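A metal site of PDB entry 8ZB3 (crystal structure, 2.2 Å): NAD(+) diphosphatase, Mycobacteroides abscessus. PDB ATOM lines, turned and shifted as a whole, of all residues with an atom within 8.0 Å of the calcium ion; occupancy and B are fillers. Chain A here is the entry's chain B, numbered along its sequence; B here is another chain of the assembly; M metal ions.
O of Glu 210 sits at hydrogen-bond distance from N of Gly 252.
ND2 of Asn 250 is in hydrogen-bond range of OD1 of Asp 251.
Of the 16 residues printed, 4 come within 4 Å of the calcium ion.
Along chain A the residues within 4 Å of the calcium ion span positions 210 to 251.
The nearest printed residue that does not touch the calcium ion is Gly 252 (4.4 Å).
The calcium ion is bound by OD2 of Asp 20 of chain B (1.9 Å).
The side-chain carboxylate (OE1) of Glu 21 of chain B binds the calcium ion (2.2 Å).
O of Asp 251 binds the calcium ion (2.2 Å).
The side-chain carboxylate (OE1) of Glu 210 binds the calcium ion, 2.3 Å away.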
ATOM      1  N   ARG A 206      31.774   5.780   7.646  1.00  0.00           N
ATOM      2  CA  ARG A 206      31.723   6.908   6.721  1.00  0.00           C
ATOM      3  C   ARG A 206      30.281   7.443   6.642  1.00  0.00           C
ATOM      4  O   ARG A 206      30.061   8.638   6.739  1.00  0.00           O
ATOM      5  CB  ARG A 206      32.278   6.506   5.352  1.00  0.00           C
ATOM      6  CG  ARG A 206      32.177   7.581   4.292  1.00  0.00           C
ATOM      7  CD  ARG A 206      32.707   7.140   2.919  1.00  0.00           C
ATOM      8  NE  ARG A 206      32.000   5.988   2.358  1.00  0.00           N
ATOM      9  CZ  ARG A 206      30.703   5.951   2.069  1.00  0.00           C
ATOM     10  NH1 ARG A 206      29.957   7.033   2.130  1.00  0.00           N
ATOM     11  NH2 ARG A 206      30.125   4.824   1.674  1.00  0.00           N
ATOM     12  N   GLU A 207      29.317   6.533   6.449  1.00  0.00           N
ATOM     13  CA  GLU A 207      27.937   6.920   6.231  1.00  0.00           C
ATOM     14  C   GLU A 207      27.327   7.568   7.481  1.00  0.00           C
ATOM     15  O   GLU A 207      26.582   8.512   7.386  1.00  0.00           O
ATOM     16  CB  GLU A 207      27.096   5.729   5.790  1.00  0.00           C
ATOM     17  CG  GLU A 207      27.350   5.310   4.351  1.00  0.00           C
ATOM     18  CD  GLU A 207      26.808   6.238   3.272  1.00  0.00           C
ATOM     19  OE1 GLU A 207      27.139   6.028   2.116  1.00  0.00           O
ATOM     20  OE2 GLU A 207      26.093   7.185   3.587  1.00  0.00           O
ATOM     21  N   ALA A 209      28.978   9.268   9.716  1.00  0.00           N
ATOM     22  CA  ALA A 209      29.602  10.585   9.749  1.00  0.00           C
ATOM     23  C   ALA A 209      28.922  11.534   8.744  1.00  0.00           C
ATOM     24  O   ALA A 209      28.597  12.654   9.109  1.00  0.00           O
ATOM     25  CB  ALA A 209      31.097  10.483   9.498  1.00  0.00           C
ATOM     26  N   GLU A 210      28.699  11.058   7.514  1.00  0.00           N
ATOM     27  CA  GLU A 210      28.068  11.857   6.471  1.00  0.00           C
ATOM     28  C   GLU A 210      26.658  12.299   6.886  1.00  0.00           C
ATOM     29  O   GLU A 210      26.247  13.403   6.576  1.00  0.00           O
ATOM     30  CB  GLU A 210      27.911  11.085   5.165  1.00  0.00           C
ATOM     31  CG  GLU A 210      29.189  10.961   4.368  1.00  0.00           C
ATOM     32  CD  GLU A 210      29.760  12.306   3.960  1.00  0.00           C
ATOM     33  OE1 GLU A 210      28.980  13.149   3.454  1.00  0.00           O
ATOM     34  OE2 GLU A 210      30.978  12.521   4.168  1.00  0.00           O
ATOM     35  N   GLU A 211      25.899  11.430   7.557  1.00  0.00           N
ATOM     36  CA  GLU A 211      24.494  11.671   7.754  1.00  0.00           C
ATOM     37  C   GLU A 211      24.239  12.495   9.015  1.00  0.00           C
ATOM     38  O   GLU A 211      23.400  13.397   9.022  1.00  0.00           O
ATOM     39  CB  GLU A 211      23.711  10.363   7.843  1.00  0.00           C
ATOM     40  CG  GLU A 211      23.803   9.537   6.555  1.00  0.00           C
ATOM     41  CD  GLU A 211      23.094  10.157   5.354  1.00  0.00           C
ATOM     42  OE1 GLU A 211      23.783  10.421   4.335  1.00  0.00           O
ATOM     43  OE2 GLU A 211      21.868  10.358   5.424  1.00  0.00           O
ATOM     44  N   PHE A 249      24.316  17.789  10.214  1.00  0.00           N
ATOM     45  CA  PHE A 249      23.513  17.186   9.170  1.00  0.00           C
ATOM     46  C   PHE A 249      23.878  17.680   7.790  1.00  0.00           C
ATOM     47  O   PHE A 249      23.217  17.233   6.863  1.00  0.00           O
ATOM     48  CB  PHE A 249      22.051  17.521   9.415  1.00  0.00           C
ATOM     49  CG  PHE A 249      21.568  17.062  10.762  1.00  0.00           C
ATOM     50  CD1 PHE A 249      21.794  15.757  11.180  1.00  0.00           C
ATOM     51  CD2 PHE A 249      20.919  17.942  11.603  1.00  0.00           C
ATOM     52  CE1 PHE A 249      21.343  15.345  12.419  1.00  0.00           C
ATOM     53  CE2 PHE A 249      20.455  17.525  12.838  1.00  0.00           C
ATOM     54  CZ  PHE A 249      20.676  16.237  13.253  1.00  0.00           C
ATOM     55  N   ASN A 250      24.843  18.596   7.654  1.00  0.00           N
ATOM     56  CA  ASN A 250      25.022  19.289   6.379  1.00  0.00           C
ATOM     57  C   ASN A 250      25.459  18.321   5.272  1.00  0.00           C
ATOM     58  O   ASN A 250      24.803  18.335   4.251  1.00  0.00           O
ATOM     59  CB  ASN A 250      25.810  20.603   6.485  1.00  0.00           C
ATOM     60  CG  ASN A 250      27.137  20.497   7.188  1.00  0.00           C
ATOM     61  OD1 ASN A 250      27.185  20.063   8.339  1.00  0.00           O
ATOM     62  ND2 ASN A 250      28.205  20.908   6.509  1.00  0.00           N
ATOM     63  N   ASP A 251      26.426  17.424   5.537  1.00  0.00           N
ATOM     64  CA  ASP A 251      26.999  16.579   4.504  1.00  0.00           C
ATOM     65  C   ASP A 251      26.019  15.478   4.037  1.00  0.00           C
ATOM     66  O   ASP A 251      26.341  14.771   3.107  1.00  0.00           O
ATOM     67  CB  ASP A 251      28.300  15.957   5.004  1.00  0.00           C
ATOM     68  CG  ASP A 251      29.540  16.833   4.888  1.00  0.00           C
ATOM     69  OD1 ASP A 251      29.404  18.082   4.984  1.00  0.00           O
ATOM     70  OD2 ASP A 251      30.649  16.255   4.709  1.00  0.00           O
ATOM     71  N   GLY A 252      24.851  15.328   4.659  1.00  0.00           N
ATOM     72  CA  GLY A 252      24.004  14.164   4.447  1.00  0.00           C
ATOM     73  C   GLY A 252      22.599  14.500   3.979  1.00  0.00           C
ATOM     74  O   GLY A 252      22.343  15.636   3.583  1.00  0.00           O
ATOM     75  N   GLU A 253      21.690  13.536   4.094  1.00  0.00           N
ATOM     76  CA  GLU A 253      20.304  13.686   3.681  1.00  0.00           C
ATOM     77  C   GLU A 253      19.392  13.649   4.900  1.00  0.00           C
ATOM     78  O   GLU A 253      18.218  13.345   4.738  1.00  0.00           O
ATOM     79  CB  GLU A 253      19.895  12.581   2.698  1.00  0.00           C
ATOM     80  CG  GLU A 253      20.043  12.999   1.225  1.00  0.00           C
ATOM     81  CD  GLU A 253      21.476  13.005   0.723  1.00  0.00           C
ATOM     82  OE1 GLU A 253      22.115  11.945   0.847  1.00  0.00           O
ATOM     83  OE2 GLU A 253      21.965  14.057   0.251  1.00  0.00           O
ATOM     84  N   ALA B  19      36.244  13.095   0.858  1.00  0.00           N
ATOM     85  CA  ALA B  19      35.782  14.454   0.601  1.00  0.00           C
ATOM     86  C   ALA B  19      34.585  14.442  -0.367  1.00  0.00           C
ATOM     87  O   ALA B  19      34.635  15.115  -1.402  1.00  0.00           O
ATOM     88  CB  ALA B  19      36.923  15.288   0.064  1.00  0.00           C
ATOM     89  N   ASP B  20      33.553  13.699   0.006  1.00  0.00           N
ATOM     90  CA  ASP B  20      32.429  13.410  -0.884  1.00  0.00           C
ATOM     91  C   ASP B  20      31.812  14.714  -1.377  1.00  0.00           C
ATOM     92  O   ASP B  20      31.468  14.822  -2.562  1.00  0.00           O
ATOM     93  CB  ASP B  20      31.408  12.521  -0.172  1.00  0.00           C
ATOM     94  CG  ASP B  20      30.690  13.219   0.960  1.00  0.00           C
ATOM     95  OD1 ASP B  20      31.361  13.708   1.950  1.00  0.00           O
ATOM     96  OD2 ASP B  20      29.467  13.281   0.875  1.00  0.00           O
ATOM     97  N   GLU B  21      31.704  15.721  -0.513  1.00  0.00           N
ATOM     98  CA  GLU B  21      30.994  16.950  -0.877  1.00  0.00           C
ATOM     99  C   GLU B  21      31.692  17.663  -2.033  1.00  0.00           C
ATOM    100  O   GLU B  21      31.003  18.367  -2.788  1.00  0.00           O
ATOM    101  CB  GLU B  21      30.805  17.875   0.327  1.00  0.00           C
ATOM    102  CG  GLU B  21      29.799  17.317   1.316  1.00  0.00           C
ATOM    103  CD  GLU B  21      28.463  17.075   0.657  1.00  0.00           C
ATOM    104  OE1 GLU B  21      27.993  15.911   0.624  1.00  0.00           O
ATOM    105  OE2 GLU B  21      27.952  18.046   0.096  1.00  0.00           O
ATOM    106  N   LEU B  22      33.002  17.452  -2.215  1.00  0.00           N
ATOM    107  CA  LEU B  22      33.692  18.104  -3.315  1.00  0.00           C
ATOM    108  C   LEU B  22      33.403  17.474  -4.674  1.00  0.00           C
ATOM    109  O   LEU B  22      33.584  18.155  -5.707  1.00  0.00           O
ATOM    110  CB  LEU B  22      35.209  18.081  -3.075  1.00  0.00           C
ATOM    111  CG  LEU B  22      35.705  18.957  -1.923  1.00  0.00           C
ATOM    112  CD1 LEU B  22      37.213  18.902  -1.800  1.00  0.00           C
ATOM    113  CD2 LEU B  22      35.249  20.390  -2.180  1.00  0.00           C
ATOM    114  N   ARG B  23      32.923  16.225  -4.690  1.00  0.00           N
ATOM    115  CA  ARG B  23      32.615  15.552  -5.936  1.00  0.00           C
ATOM    116  C   ARG B  23      31.558  16.310  -6.728  1.00  0.00           C
ATOM    117  O   ARG B  23      31.622  16.345  -7.964  1.00  0.00           O
ATOM    118  CB  ARG B  23      32.077  14.125  -5.692  1.00  0.00           C
ATOM    119  CG  ARG B  23      33.067  13.158  -5.039  1.00  0.00           C
ATOM    120  CD  ARG B  23      32.299  11.972  -4.481  1.00  0.00           C
ATOM    121  NE  ARG B  23      33.182  10.990  -3.891  1.00  0.00           N
ATOM    122  CZ  ARG B  23      32.787   9.853  -3.315  1.00  0.00           C
ATOM    123  NH1 ARG B  23      31.496   9.563  -3.237  1.00  0.00           N
ATOM    124  NH2 ARG B  23      33.681   9.008  -2.839  1.00  0.00           N
ATOM    125  N   SER B  24      30.570  16.880  -6.013  1.00  0.00           N
ATOM    126  CA  SER B  24      29.478  17.620  -6.608  1.00  0.00           C
ATOM    127  C   SER B  24      29.758  19.122  -6.670  1.00  0.00           C
ATOM    128  O   SER B  24      28.841  19.892  -6.910  1.00  0.00           O
ATOM    129  CB  SER B  24      28.214  17.357  -5.834  1.00  0.00           C
ATOM    130  OG  SER B  24      27.900  15.978  -5.856  1.00  0.00           O
HETATM  131 CA    CA M   1      27.833  13.970   1.667  1.00  0.00          CA
